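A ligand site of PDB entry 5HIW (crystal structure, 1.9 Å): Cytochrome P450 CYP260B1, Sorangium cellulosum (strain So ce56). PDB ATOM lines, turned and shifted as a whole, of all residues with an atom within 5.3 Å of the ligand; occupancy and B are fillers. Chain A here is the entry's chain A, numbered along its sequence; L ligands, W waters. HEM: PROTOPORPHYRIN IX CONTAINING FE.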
ATOM      1  N   LEU A  52     -13.807  -5.291  28.728  1.00  0.00           N
ATOM      2  CA  LEU A  52     -14.584  -6.343  28.001  1.00  0.00           C
ATOM      3  C   LEU A  52     -13.689  -7.190  27.037  1.00  0.00           C
ATOM      4  O   LEU A  52     -13.945  -8.371  26.851  1.00  0.00           O
ATOM      5  CB  LEU A  52     -15.722  -5.681  27.219  1.00  0.00           C
ATOM      6  CG  LEU A  52     -16.874  -5.104  28.065  1.00  0.00           C
ATOM      7  CD1 LEU A  52     -17.797  -4.331  27.126  1.00  0.00           C
ATOM      8  CD2 LEU A  52     -17.570  -6.207  28.893  1.00  0.00           C
ATOM      9  N   THR A  60     -16.346 -13.683  34.036  1.00  0.00           N
ATOM     10  CA  THR A  60     -17.745 -13.666  34.412  1.00  0.00           C
ATOM     11  C   THR A  60     -18.029 -14.548  35.634  1.00  0.00           C
ATOM     12  O   THR A  60     -19.127 -15.055  35.834  1.00  0.00           O
ATOM     13  CB  THR A  60     -18.627 -14.020  33.180  1.00  0.00           C
ATOM     14  OG1 THR A  60     -18.152 -15.210  32.540  1.00  0.00           O
ATOM     15  CG2 THR A  60     -18.666 -12.866  32.199  1.00  0.00           C
ATOM     16  N   TYR A  63     -21.179 -14.362  37.889  1.00  0.00           N
ATOM     17  CA  TYR A  63     -22.463 -14.844  37.389  1.00  0.00           C
ATOM     18  C   TYR A  63     -22.662 -16.315  37.687  1.00  0.00           C
ATOM     19  O   TYR A  63     -23.768 -16.792  37.546  1.00  0.00           O
ATOM     20  CB  TYR A  63     -22.577 -14.793  35.861  1.00  0.00           C
ATOM     21  CG  TYR A  63     -22.943 -13.506  35.147  1.00  0.00           C
ATOM     22  CD1 TYR A  63     -24.266 -13.021  35.098  1.00  0.00           C
ATOM     23  CD2 TYR A  63     -21.994 -12.861  34.356  1.00  0.00           C
ATOM     24  CE1 TYR A  63     -24.589 -11.861  34.379  1.00  0.00           C
ATOM     25  CE2 TYR A  63     -22.312 -11.723  33.618  1.00  0.00           C
ATOM     26  CZ  TYR A  63     -23.589 -11.219  33.630  1.00  0.00           C
ATOM     27  OH  TYR A  63     -23.858 -10.102  32.852  1.00  0.00           O
ATOM     28  N   LEU A  72     -24.182 -20.212  29.588  1.00  0.00           N
ATOM     29  CA  LEU A  72     -23.365 -19.571  28.546  1.00  0.00           C
ATOM     30  C   LEU A  72     -22.477 -18.382  28.997  1.00  0.00           C
ATOM     31  O   LEU A  72     -21.250 -18.336  28.727  1.00  0.00           O
ATOM     32  CB  LEU A  72     -24.280 -19.215  27.373  1.00  0.00           C
ATOM     33  CG  LEU A  72     -23.639 -18.466  26.213  1.00  0.00           C
ATOM     34  CD1 LEU A  72     -22.665 -19.347  25.471  1.00  0.00           C
ATOM     35  CD2 LEU A  72     -24.629 -17.938  25.222  1.00  0.00           C
ATOM     36  N   VAL A  73     -23.089 -17.416  29.658  1.00  0.00           N
ATOM     37  CA  VAL A  73     -22.369 -16.229  30.046  1.00  0.00           C
ATOM     38  C   VAL A  73     -21.247 -16.417  31.067  1.00  0.00           C
ATOM     39  O   VAL A  73     -20.396 -15.581  31.186  1.00  0.00           O
ATOM     40  CB  VAL A  73     -23.358 -15.142  30.551  1.00  0.00           C
ATOM     41  CG1 VAL A  73     -23.839 -15.461  31.951  1.00  0.00           C
ATOM     42  CG2 VAL A  73     -22.691 -13.767  30.530  1.00  0.00           C
ATOM     43  N   HIS A  80     -17.001 -21.773  25.869  1.00  0.00           N
ATOM     44  CA  HIS A  80     -17.916 -20.708  25.433  1.00  0.00           C
ATOM     45  C   HIS A  80     -18.035 -20.761  23.940  1.00  0.00           C
ATOM     46  O   HIS A  80     -19.115 -20.630  23.386  1.00  0.00           O
ATOM     47  CB  HIS A  80     -17.466 -19.341  25.900  1.00  0.00           C
ATOM     48  CG  HIS A  80     -18.351 -18.243  25.423  1.00  0.00           C
ATOM     49  ND1 HIS A  80     -18.109 -17.528  24.263  1.00  0.00           N
ATOM     50  CD2 HIS A  80     -19.526 -17.750  25.935  1.00  0.00           C
ATOM     51  CE1 HIS A  80     -19.090 -16.650  24.074  1.00  0.00           C
ATOM     52  NE2 HIS A  80     -19.956 -16.772  25.056  1.00  0.00           N
ATOM     53  N   ARG A  84     -21.634 -21.062  22.372  1.00  0.00           N
ATOM     54  CA  ARG A  84     -21.990 -19.884  21.610  1.00  0.00           C
ATOM     55  C   ARG A  84     -22.378 -20.171  20.154  1.00  0.00           C
ATOM     56  O   ARG A  84     -23.277 -19.539  19.571  1.00  0.00           O
ATOM     57  CB  ARG A  84     -20.863 -18.814  21.706  1.00  0.00           C
ATOM     58  CG  ARG A  84     -21.142 -17.498  20.950  1.00  0.00           C
ATOM     59  CD  ARG A  84     -22.406 -16.822  21.484  1.00  0.00           C
ATOM     60  NE  ARG A  84     -22.669 -15.583  20.751  1.00  0.00           N
ATOM     61  CZ  ARG A  84     -22.626 -14.335  21.240  1.00  0.00           C
ATOM     62  NH1 ARG A  84     -22.410 -14.064  22.514  1.00  0.00           N
ATOM     63  NH2 ARG A  84     -22.884 -13.342  20.415  1.00  0.00           N
ATOM     64  N   PHE A  87     -25.995 -21.384  20.242  1.00  0.00           N
ATOM     65  CA  PHE A  87     -26.891 -20.169  20.334  1.00  0.00           C
ATOM     66  C   PHE A  87     -26.933 -19.349  19.074  1.00  0.00           C
ATOM     67  O   PHE A  87     -27.973 -18.910  18.670  1.00  0.00           O
ATOM     68  CB  PHE A  87     -26.509 -19.328  21.568  1.00  0.00           C
ATOM     69  CG  PHE A  87     -26.908 -19.932  22.887  1.00  0.00           C
ATOM     70  CD1 PHE A  87     -26.189 -20.959  23.473  1.00  0.00           C
ATOM     71  CD2 PHE A  87     -28.046 -19.487  23.539  1.00  0.00           C
ATOM     72  CE1 PHE A  87     -26.507 -21.503  24.687  1.00  0.00           C
ATOM     73  CE2 PHE A  87     -28.415 -20.032  24.757  1.00  0.00           C
ATOM     74  CZ  PHE A  87     -27.649 -21.035  25.358  1.00  0.00           C
ATOM     75  N   LEU A  91     -30.398 -18.288  16.570  1.00  0.00           N
ATOM     76  CA  LEU A  91     -30.812 -16.912  16.463  1.00  0.00           C
ATOM     77  C   LEU A  91     -30.267 -16.208  15.179  1.00  0.00           C
ATOM     78  O   LEU A  91     -30.057 -14.950  15.139  1.00  0.00           O
ATOM     79  CB  LEU A  91     -30.343 -16.133  17.681  1.00  0.00           C
ATOM     80  CG  LEU A  91     -31.060 -16.553  18.934  1.00  0.00           C
ATOM     81  CD1 LEU A  91     -30.281 -16.180  20.187  1.00  0.00           C
ATOM     82  CD2 LEU A  91     -32.473 -16.052  18.983  1.00  0.00           C
ATOM     83  N   THR A 224     -31.911 -20.326  29.366  1.00  0.00           N
ATOM     84  CA  THR A 224     -30.975 -19.208  29.164  1.00  0.00           C
ATOM     85  C   THR A 224     -31.569 -18.100  28.312  1.00  0.00           C
ATOM     86  O   THR A 224     -31.389 -16.874  28.695  1.00  0.00           O
ATOM     87  CB  THR A 224     -29.622 -19.689  28.639  1.00  0.00           C
ATOM     88  OG1 THR A 224     -28.981 -20.430  29.679  1.00  0.00           O
ATOM     89  CG2 THR A 224     -28.734 -18.599  28.214  1.00  0.00           C
ATOM     90  N   LEU A 225     -32.296 -18.460  27.252  1.00  0.00           N
ATOM     91  CA  LEU A 225     -32.903 -17.480  26.409  1.00  0.00           C
ATOM     92  C   LEU A 225     -34.036 -16.738  27.145  1.00  0.00           C
ATOM     93  O   LEU A 225     -34.216 -15.530  26.936  1.00  0.00           O
ATOM     94  CB  LEU A 225     -33.448 -18.052  25.127  1.00  0.00           C
ATOM     95  CG  LEU A 225     -32.301 -18.730  24.247  1.00  0.00           C
ATOM     96  CD1 LEU A 225     -32.895 -19.386  23.032  1.00  0.00           C
ATOM     97  CD2 LEU A 225     -31.226 -17.702  23.874  1.00  0.00           C
ATOM     98  N   GLY A 228     -32.471 -14.326  29.660  1.00  0.00           N
ATOM     99  CA  GLY A 228     -31.820 -13.201  28.990  1.00  0.00           C
ATOM    100  C   GLY A 228     -32.744 -12.236  28.299  1.00  0.00           C
ATOM    101  O   GLY A 228     -32.354 -11.087  28.089  1.00  0.00           O
ATOM    102  N   SER A 229     -33.980 -12.651  27.963  1.00  0.00           N
ATOM    103  CA  SER A 229     -34.894 -11.803  27.212  1.00  0.00           C
ATOM    104  C   SER A 229     -36.103 -11.263  27.934  1.00  0.00           C
ATOM    105  O   SER A 229     -36.666 -10.282  27.453  1.00  0.00           O
ATOM    106  CB  SER A 229     -35.498 -12.576  26.043  1.00  0.00           C
ATOM    107  OG  SER A 229     -36.216 -13.756  26.525  1.00  0.00           O
ATOM    108  N   THR A 232     -35.385  -7.839  29.917  1.00  0.00           N
ATOM    109  CA  THR A 232     -34.595  -6.941  29.047  1.00  0.00           C
ATOM    110  C   THR A 232     -35.478  -6.401  27.955  1.00  0.00           C
ATOM    111  O   THR A 232     -35.435  -5.206  27.646  1.00  0.00           O
ATOM    112  CB  THR A 232     -33.352  -7.642  28.455  1.00  0.00           C
ATOM    113  OG1 THR A 232     -33.782  -8.862  27.798  1.00  0.00           O
ATOM    114  CG2 THR A 232     -32.278  -7.991  29.536  1.00  0.00           C
ATOM    115  N   THR A 233     -36.261  -7.273  27.287  1.00  0.00           N
ATOM    116  CA  THR A 233     -37.076  -6.851  26.216  1.00  0.00           C
ATOM    117  C   THR A 233     -38.012  -5.704  26.611  1.00  0.00           C
ATOM    118  O   THR A 233     -38.206  -4.770  25.837  1.00  0.00           O
ATOM    119  CB  THR A 233     -37.928  -8.045  25.647  1.00  0.00           C
ATOM    120  OG1 THR A 233     -37.030  -9.062  25.178  1.00  0.00           O
ATOM    121  CG2 THR A 233     -38.745  -7.549  24.503  1.00  0.00           C
ATOM    122  N   MET A 236     -36.038  -2.372  26.979  1.00  0.00           N
ATOM    123  CA  MET A 236     -35.723  -1.830  25.614  1.00  0.00           C
ATOM    124  C   MET A 236     -36.903  -1.236  24.914  1.00  0.00           C
ATOM    125  O   MET A 236     -36.841  -0.140  24.330  1.00  0.00           O
ATOM    126  CB  MET A 236     -35.093  -2.915  24.725  1.00  0.00           C
ATOM    127  CG  MET A 236     -34.966  -2.501  23.219  1.00  0.00           C
ATOM    128  SD  MET A 236     -33.743  -3.576  22.409  1.00  0.00           S
ATOM    129  CE  MET A 236     -33.629  -2.719  20.833  1.00  0.00           C
ATOM    130  N   SER A 274     -31.429   1.030  28.049  1.00  0.00           N
ATOM    131  CA  SER A 274     -31.972   0.393  29.239  1.00  0.00           C
ATOM    132  C   SER A 274     -30.991  -0.422  30.039  1.00  0.00           C
ATOM    133  O   SER A 274     -31.339  -0.889  31.128  1.00  0.00           O
ATOM    134  CB  SER A 274     -33.129  -0.529  28.910  1.00  0.00           C
ATOM    135  OG  SER A 274     -32.818  -1.366  27.837  1.00  0.00           O
ATOM    136  N   ALA A 275     -29.809  -0.691  29.488  1.00  0.00           N
ATOM    137  CA  ALA A 275     -28.822  -1.528  30.142  1.00  0.00           C
ATOM    138  C   ALA A 275     -27.867  -0.593  30.815  1.00  0.00           C
ATOM    139  O   ALA A 275     -27.007  -0.042  30.162  1.00  0.00           O
ATOM    140  CB  ALA A 275     -28.054  -2.256  29.100  1.00  0.00           C
ATOM    141  N   ILE A 278     -22.903  -3.981  33.655  1.00  0.00           N
ATOM    142  CA  ILE A 278     -22.628  -5.371  33.833  1.00  0.00           C
ATOM    143  C   ILE A 278     -21.420  -5.507  34.730  1.00  0.00           C
ATOM    144  O   ILE A 278     -20.630  -4.535  34.923  1.00  0.00           O
ATOM    145  CB  ILE A 278     -22.370  -6.118  32.517  1.00  0.00           C
ATOM    146  CG1 ILE A 278     -21.374  -5.366  31.704  1.00  0.00           C
ATOM    147  CG2 ILE A 278     -23.664  -6.373  31.783  1.00  0.00           C
ATOM    148  CD1 ILE A 278     -21.130  -5.960  30.339  1.00  0.00           C
ATOM    149  N   VAL A 279     -21.237  -6.720  35.229  1.00  0.00           N
ATOM    150  CA  VAL A 279     -20.281  -6.949  36.248  1.00  0.00           C
ATOM    151  C   VAL A 279     -19.190  -7.947  35.752  1.00  0.00           C
ATOM    152  O   VAL A 279     -19.484  -8.845  34.965  1.00  0.00           O
ATOM    153  CB  VAL A 279     -20.998  -7.542  37.462  1.00  0.00           C
ATOM    154  CG1 VAL A 279     -19.968  -7.925  38.483  1.00  0.00           C
ATOM    155  CG2 VAL A 279     -22.032  -6.532  38.013  1.00  0.00           C
ATOM    156  N   ARG A 280     -17.953  -7.705  36.176  1.00  0.00           N
ATOM    157  CA  ARG A 280     -16.784  -8.627  35.989  1.00  0.00           C
ATOM    158  C   ARG A 280     -16.050  -8.903  37.309  1.00  0.00           C
ATOM    159  O   ARG A 280     -16.193  -8.143  38.286  1.00  0.00           O
ATOM    160  CB  ARG A 280     -15.842  -8.001  34.975  1.00  0.00           C
ATOM    161  CG  ARG A 280     -16.438  -7.804  33.554  1.00  0.00           C
ATOM    162  CD  ARG A 280     -16.557  -9.171  32.886  1.00  0.00           C
ATOM    163  NE  ARG A 280     -17.008  -9.228  31.513  1.00  0.00           N
ATOM    164  CZ  ARG A 280     -18.295  -9.294  31.111  1.00  0.00           C
ATOM    165  NH1 ARG A 280     -18.570  -9.376  29.818  1.00  0.00           N
ATOM    166  NH2 ARG A 280     -19.275  -9.199  31.984  1.00  0.00           N
ATOM    167  N   LEU A 303     -22.473   0.863  30.968  1.00  0.00           N
ATOM    168  CA  LEU A 303     -22.792   0.722  29.547  1.00  0.00           C
ATOM    169  C   LEU A 303     -23.476   1.974  29.031  1.00  0.00           C
ATOM    170  O   LEU A 303     -23.908   1.987  27.898  1.00  0.00           O
ATOM    171  CB  LEU A 303     -23.611  -0.529  29.336  1.00  0.00           C
ATOM    172  CG  LEU A 303     -22.978  -1.843  29.778  1.00  0.00           C
ATOM    173  CD1 LEU A 303     -23.888  -3.060  29.593  1.00  0.00           C
ATOM    174  CD2 LEU A 303     -21.663  -2.177  29.133  1.00  0.00           C
ATOM    175  N   LEU A 329     -22.967   0.319  23.806  1.00  0.00           N
ATOM    176  CA  LEU A 329     -22.565  -0.699  24.739  1.00  0.00           C
ATOM    177  C   LEU A 329     -23.782  -1.451  25.297  1.00  0.00           C
ATOM    178  O   LEU A 329     -23.611  -2.228  26.248  1.00  0.00           O
ATOM    179  CB  LEU A 329     -21.842  -0.042  25.901  1.00  0.00           C
ATOM    180  CG  LEU A 329     -20.418   0.487  25.520  1.00  0.00           C
ATOM    181  CD1 LEU A 329     -19.825   1.204  26.686  1.00  0.00           C
ATOM    182  CD2 LEU A 329     -19.477  -0.552  25.019  1.00  0.00           C
ATOM    183  N   ASN A 330     -24.970  -1.107  24.821  1.00  0.00           N
ATOM    184  CA  ASN A 330     -26.243  -1.684  25.386  1.00  0.00           C
ATOM    185  C   ASN A 330     -26.276  -3.184  25.318  1.00  0.00           C
ATOM    186  O   ASN A 330     -26.937  -3.756  26.124  1.00  0.00           O
ATOM    187  CB  ASN A 330     -27.498  -1.080  24.769  1.00  0.00           C
ATOM    188  CG  ASN A 330     -27.570  -1.240  23.250  1.00  0.00           C
ATOM    189  OD1 ASN A 330     -26.657  -0.874  22.553  1.00  0.00           O
ATOM    190  ND2 ASN A 330     -28.666  -1.801  22.747  1.00  0.00           N
ATOM    191  N   PHE A 331     -25.624  -3.808  24.309  1.00  0.00           N
ATOM    192  CA  PHE A 331     -25.566  -5.245  24.176  1.00  0.00           C
ATOM    193  C   PHE A 331     -24.187  -5.756  24.595  1.00  0.00           C
ATOM    194  O   PHE A 331     -23.815  -6.880  24.310  1.00  0.00           O
ATOM    195  CB  PHE A 331     -25.895  -5.615  22.712  1.00  0.00           C
ATOM    196  CG  PHE A 331     -27.318  -5.417  22.291  1.00  0.00           C
ATOM    197  CD1 PHE A 331     -28.364  -5.979  22.999  1.00  0.00           C
ATOM    198  CD2 PHE A 331     -27.620  -4.706  21.138  1.00  0.00           C
ATOM    199  CE1 PHE A 331     -29.688  -5.792  22.577  1.00  0.00           C
ATOM    200  CE2 PHE A 331     -28.920  -4.481  20.741  1.00  0.00           C
ATOM    201  CZ  PHE A 331     -29.963  -5.059  21.416  1.00  0.00           C
ATOM    202  N   GLY A 332     -23.396  -4.920  25.269  1.00  0.00           N
ATOM    203  CA  GLY A 332     -22.098  -5.362  25.708  1.00  0.00           C
ATOM    204  C   GLY A 332     -21.076  -5.264  24.586  1.00  0.00           C
ATOM    205  O   GLY A 332     -21.180  -4.390  23.693  1.00  0.00           O
ATOM    206  N   LEU A 335     -16.437 -11.108  23.910  1.00  0.00           N
ATOM    207  CA  LEU A 335     -16.845 -12.536  23.957  1.00  0.00           C
ATOM    208  C   LEU A 335     -18.346 -12.755  24.224  1.00  0.00           C
ATOM    209  O   LEU A 335     -19.074 -13.558  23.609  1.00  0.00           O
ATOM    210  CB  LEU A 335     -16.060 -13.151  25.157  1.00  0.00           C
ATOM    211  CG  LEU A 335     -16.172 -14.622  25.517  1.00  0.00           C
ATOM    212  CD1 LEU A 335     -15.752 -15.374  24.261  1.00  0.00           C
ATOM    213  CD2 LEU A 335     -15.320 -15.128  26.717  1.00  0.00           C
ATOM    214  N   HIS A 336     -18.816 -12.033  25.232  1.00  0.00           N
ATOM    215  CA  HIS A 336     -20.173 -12.193  25.697  1.00  0.00           C
ATOM    216  C   HIS A 336     -21.169 -11.218  25.114  1.00  0.00           C
ATOM    217  O   HIS A 336     -22.310 -11.157  25.604  1.00  0.00           O
ATOM    218  CB  HIS A 336     -20.173 -12.128  27.224  1.00  0.00           C
ATOM    219  CG  HIS A 336     -19.406 -13.243  27.864  1.00  0.00           C
ATOM    220  ND1 HIS A 336     -19.872 -14.547  27.884  1.00  0.00           N
ATOM    221  CD2 HIS A 336     -18.197 -13.260  28.478  1.00  0.00           C
ATOM    222  CE1 HIS A 336     -18.967 -15.311  28.487  1.00  0.00           C
ATOM    223  NE2 HIS A 336     -17.977 -14.567  28.911  1.00  0.00           N
ATOM    224  N   TYR A 337     -20.864 -10.542  23.992  1.00  0.00           N
ATOM    225  CA  TYR A 337     -21.795  -9.639  23.334  1.00  0.00           C
ATOM    226  C   TYR A 337     -23.129 -10.330  23.171  1.00  0.00           C
ATOM    227  O   TYR A 337     -23.207 -11.507  22.833  1.00  0.00           O
ATOM    228  CB  TYR A 337     -21.284  -9.186  21.911  1.00  0.00           C
ATOM    229  CG  TYR A 337     -22.195  -8.259  21.160  1.00  0.00           C
ATOM    230  CD1 TYR A 337     -23.224  -8.767  20.311  1.00  0.00           C
ATOM    231  CD2 TYR A 337     -22.042  -6.904  21.221  1.00  0.00           C
ATOM    232  CE1 TYR A 337     -24.013  -7.916  19.541  1.00  0.00           C
ATOM    233  CE2 TYR A 337     -22.874  -6.068  20.472  1.00  0.00           C
ATOM    234  CZ  TYR A 337     -23.821  -6.571  19.649  1.00  0.00           C
ATOM    235  OH  TYR A 337     -24.673  -5.711  18.945  1.00  0.00           O
ATOM    236  N   CYS A 338     -24.208  -9.638  23.511  1.00  0.00           N
ATOM    237  CA  CYS A 338     -25.545 -10.276  23.543  1.00  0.00           C
ATOM    238  C   CYS A 338     -25.925 -11.102  22.332  1.00  0.00           C
ATOM    239  O   CYS A 338     -26.031 -10.608  21.232  1.00  0.00           O
ATOM    240  CB  CYS A 338     -26.642  -9.211  23.731  1.00  0.00           C
ATOM    241  SG  CYS A 338     -28.308  -9.859  23.894  1.00  0.00           S
ATOM    242  N   VAL A 339     -26.078 -12.420  22.535  1.00  0.00           N
ATOM    243  CA  VAL A 339     -26.486 -13.303  21.449  1.00  0.00           C
ATOM    244  C   VAL A 339     -27.910 -13.127  21.017  1.00  0.00           C
ATOM    245  O   VAL A 339     -28.338 -13.461  19.875  1.00  0.00           O
ATOM    246  CB  VAL A 339     -26.214 -14.778  21.895  1.00  0.00           C
ATOM    247  CG1 VAL A 339     -27.272 -15.203  22.904  1.00  0.00           C
ATOM    248  CG2 VAL A 339     -26.145 -15.688  20.683  1.00  0.00           C
ATOM    249  N   GLY A 340     -28.716 -12.550  21.915  1.00  0.00           N
ATOM    250  CA  GLY A 340     -30.079 -12.201  21.627  1.00  0.00           C
ATOM    251  C   GLY A 340     -30.442 -10.894  20.891  1.00  0.00           C
ATOM    252  O   GLY A 340     -31.609 -10.607  20.639  1.00  0.00           O
ATOM    253  N   ALA A 341     -29.446 -10.050  20.688  1.00  0.00           N
ATOM    254  CA  ALA A 341     -29.612  -8.776  20.011  1.00  0.00           C
ATOM    255  C   ALA A 341     -30.439  -8.835  18.707  1.00  0.00           C
ATOM    256  O   ALA A 341     -31.282  -7.968  18.507  1.00  0.00           O
ATOM    257  CB  ALA A 341     -28.247  -8.134  19.788  1.00  0.00           C
ATOM    258  N   LEU A 343     -32.985 -10.783  18.093  1.00  0.00           N
ATOM    259  CA  LEU A 343     -34.410 -10.949  18.506  1.00  0.00           C
ATOM    260  C   LEU A 343     -34.905  -9.656  19.096  1.00  0.00           C
ATOM    261  O   LEU A 343     -36.030  -9.234  18.829  1.00  0.00           O
ATOM    262  CB  LEU A 343     -34.568 -12.124  19.489  1.00  0.00           C
ATOM    263  CG  LEU A 343     -35.984 -12.279  20.082  1.00  0.00           C
ATOM    264  CD1 LEU A 343     -37.056 -12.426  18.998  1.00  0.00           C
ATOM    265  CD2 LEU A 343     -35.917 -13.487  20.977  1.00  0.00           C
ATOM    266  N   ALA A 344     -34.091  -9.027  19.965  1.00  0.00           N
ATOM    267  CA  ALA A 344     -34.487  -7.745  20.555  1.00  0.00           C
ATOM    268  C   ALA A 344     -34.773  -6.710  19.492  1.00  0.00           C
ATOM    269  O   ALA A 344     -35.794  -6.020  19.507  1.00  0.00           O
ATOM    270  CB  ALA A 344     -33.407  -7.324  21.482  1.00  0.00           C
HETATM  271  CHA HEM L   1     -25.691 -11.128  26.977  1.00  0.00           C
HETATM  272  CHB HEM L   1     -28.177  -6.949  27.014  1.00  0.00           C
HETATM  273  CHC HEM L   1     -31.878  -9.136  24.865  1.00  0.00           C
HETATM  274  CHD HEM L   1     -29.768 -13.338  25.744  1.00  0.00           C
HETATM  275  C1A HEM L   1     -26.000  -9.805  27.118  1.00  0.00           C
HETATM  276  C2A HEM L   1     -25.137  -8.791  27.618  1.00  0.00           C
HETATM  277  C3A HEM L   1     -25.822  -7.611  27.591  1.00  0.00           C
HETATM  278  C4A HEM L   1     -27.161  -7.912  27.180  1.00  0.00           C
HETATM  279  CMA HEM L   1     -25.279  -6.241  28.065  1.00  0.00           C
HETATM  280  CAA HEM L   1     -23.663  -8.970  27.964  1.00  0.00           C
HETATM  281  CBA HEM L   1     -23.527  -9.588  29.364  1.00  0.00           C
HETATM  282  CGA HEM L   1     -22.132  -9.548  29.877  1.00  0.00           C
HETATM  283  O1A HEM L   1     -21.166  -9.313  29.076  1.00  0.00           O
HETATM  284  O2A HEM L   1     -21.928  -9.549  31.119  1.00  0.00           O
HETATM  285  C1B HEM L   1     -29.400  -7.175  26.494  1.00  0.00           C
HETATM  286  C2B HEM L   1     -30.324  -6.116  26.216  1.00  0.00           C
HETATM  287  C3B HEM L   1     -31.371  -6.754  25.581  1.00  0.00           C
HETATM  288  C4B HEM L   1     -31.087  -8.186  25.523  1.00  0.00           C
HETATM  289  CMB HEM L   1     -30.272  -4.614  26.561  1.00  0.00           C
HETATM  290  CAB HEM L   1     -32.558  -6.029  25.186  1.00  0.00           C
HETATM  291  CBB HEM L   1     -33.728  -6.448  24.866  1.00  0.00           C
HETATM  292  C1C HEM L   1     -31.627 -10.507  24.912  1.00  0.00           C
HETATM  293  C2C HEM L   1     -32.521 -11.462  24.333  1.00  0.00           C
HETATM  294  C3C HEM L   1     -31.912 -12.659  24.606  1.00  0.00           C
HETATM  295  C4C HEM L   1     -30.716 -12.428  25.354  1.00  0.00           C
HETATM  296  CMC HEM L   1     -33.795 -11.026  23.642  1.00  0.00           C
HETATM  297  CAC HEM L   1     -32.366 -14.007  24.229  1.00  0.00           C
HETATM  298  CBC HEM L   1     -33.095 -14.192  23.138  1.00  0.00           C
HETATM  299  C1D HEM L   1     -28.477 -13.024  26.151  1.00  0.00           C
HETATM  300  C2D HEM L   1     -27.506 -14.118  26.423  1.00  0.00           C
HETATM  301  C3D HEM L   1     -26.378 -13.515  26.769  1.00  0.00           C
HETATM  302  C4D HEM L   1     -26.648 -12.070  26.673  1.00  0.00           C
HETATM  303  CMD HEM L   1     -27.767 -15.608  26.407  1.00  0.00           C
HETATM  304  CAD HEM L   1     -25.010 -14.160  27.082  1.00  0.00           C
HETATM  305  CBD HEM L   1     -24.207 -14.199  25.803  1.00  0.00           C
HETATM  306  CGD HEM L   1     -22.833 -14.859  25.981  1.00  0.00           C
HETATM  307  O1D HEM L   1     -22.267 -14.947  27.103  1.00  0.00           O
HETATM  308  O2D HEM L   1     -22.208 -15.328  24.974  1.00  0.00           O
HETATM  309  NA  HEM L   1     -27.248  -9.211  26.830  1.00  0.00           N
HETATM  310  NB  HEM L   1     -29.844  -8.340  25.953  1.00  0.00           N
HETATM  311  NC  HEM L   1     -30.549 -11.057  25.446  1.00  0.00           N
HETATM  312  ND  HEM L   1     -27.914 -11.805  26.341  1.00  0.00           N
HETATM  313 FE   HEM L   1     -28.840 -10.112  26.119  1.00  0.00          FE
HETATM  314  O   HOH W   1     -20.355  -8.283  26.777  1.00  0.00           O
HETATM  315  O   HOH W   2     -29.623 -10.335  28.266  1.00  0.00           O
HETATM  316  O   HOH W   3     -27.231 -14.694  29.849  1.00  0.00           O
HETATM  317  O   HOH W   4     -33.029  -3.897  28.318  1.00  0.00           O
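SG of Cys 338 binds FE of the ligand (2.3 Å). A ring nitrogen (ND1) of His 336 is in hydrogen-bond range of an oxygen (O1D) of the ligand. O2A of the ligand sits at hydrogen-bond distance from OH of Tyr 63 (2.7 Å). An oxygen (O2D) of the ligand sits at hydrogen-bond distance from a ring nitrogen (NE2) of His 80, 2.7 Å away. The guanidinium group of Arg 280 is in salt-bridge range of an oxygen (O1A) of the ligand, 2.7 Å away. The guanidinium group of Arg 84 lies within salt-bridge range of an oxygen (O2D) of the ligand.
N of Gly 340 lies close to SG of Cys 338, 3.4 Å away. O of Phe 331 sits at hydrogen-bond distance from N of Cys 338 (2.9 Å). The backbone carbonyl oxygen (O) of Val 73 sits close to a ring nitrogen (NE2) of His 336, 3.5 Å away. NH1 of Arg 84 sits at hydrogen-bond distance from O of Tyr 337. The side-chain hydroxyl (OG1) of Thr 60 lies within hydrogen-bond range of the backbone carbonyl oxygen (O) of Val 73. OG1 of Thr 232 sits close to O of Ser 229, at 3.2 Å. O of Leu 225 lies within hydrogen-bond range of OG of Ser 229 (2.7 Å). The backbone NH of Met 236 lies within hydrogen-bond range of the side-chain hydroxyl of Ser 274 (3.5 Å).
NC of the ligand sits close to O of Gly 228 (3.2 Å). CD2 of Leu 72 touches O2D of the ligand, at 3.6 Å. Val 73 touches the ligand. Thr 224 touches the ligand (CG2 to CMD, 3.6 Å). O of Leu 225 touches CAC of the ligand, 3.6 Å away. Ser 229 touches the ligand (CB to CMC, 3.3 Å). Thr 232 touches the ligand. Thr 233 touches the ligand. Met 236 touches the ligand (SD to CBB, 3.8 Å). Ile 278 touches the ligand. Leu 303 touches the ligand (CD1 to CMA, 3.8 Å). Asn 330 touches the ligand. CE1 of Phe 331 touches C3B of the ligand, at 3.6 Å. Gly 332 touches the ligand (N to CMA, 3.6 Å). O of Leu 335 touches O2D of the ligand (3.8 Å). Val 339 touches the ligand (CG1 to CMD, 3.6 Å). Gly 340 touches the ligand (CA to C3C, 3.5 Å). CD2 of Leu 343 touches CBC of the ligand, at 3.6 Å. Ala 344 touches the ligand. 25 residues have an atom within 4 Å of the ligand: Tyr 63, Leu 72, Val 73, His 80, Arg 84, Thr 224, Leu 225, Gly 228, Ser 229, Thr 232, Thr 233, Met 236, Ile 278, Arg 280, Leu 303, Asn 330, Phe 331, Gly 332, Leu 335, His 336, Cys 338, Val 339, Gly 340, Leu 343 and Ala 344. Along chain A the residues within 4 Å of the ligand span positions 63 to 344.
Water W4 lies within hydrogen-bond range of the side-chain hydroxyl (OG) of Ser 274 (2.6 Å) and the backbone carbonyl oxygen (O) of Thr 232 (2.8 Å).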
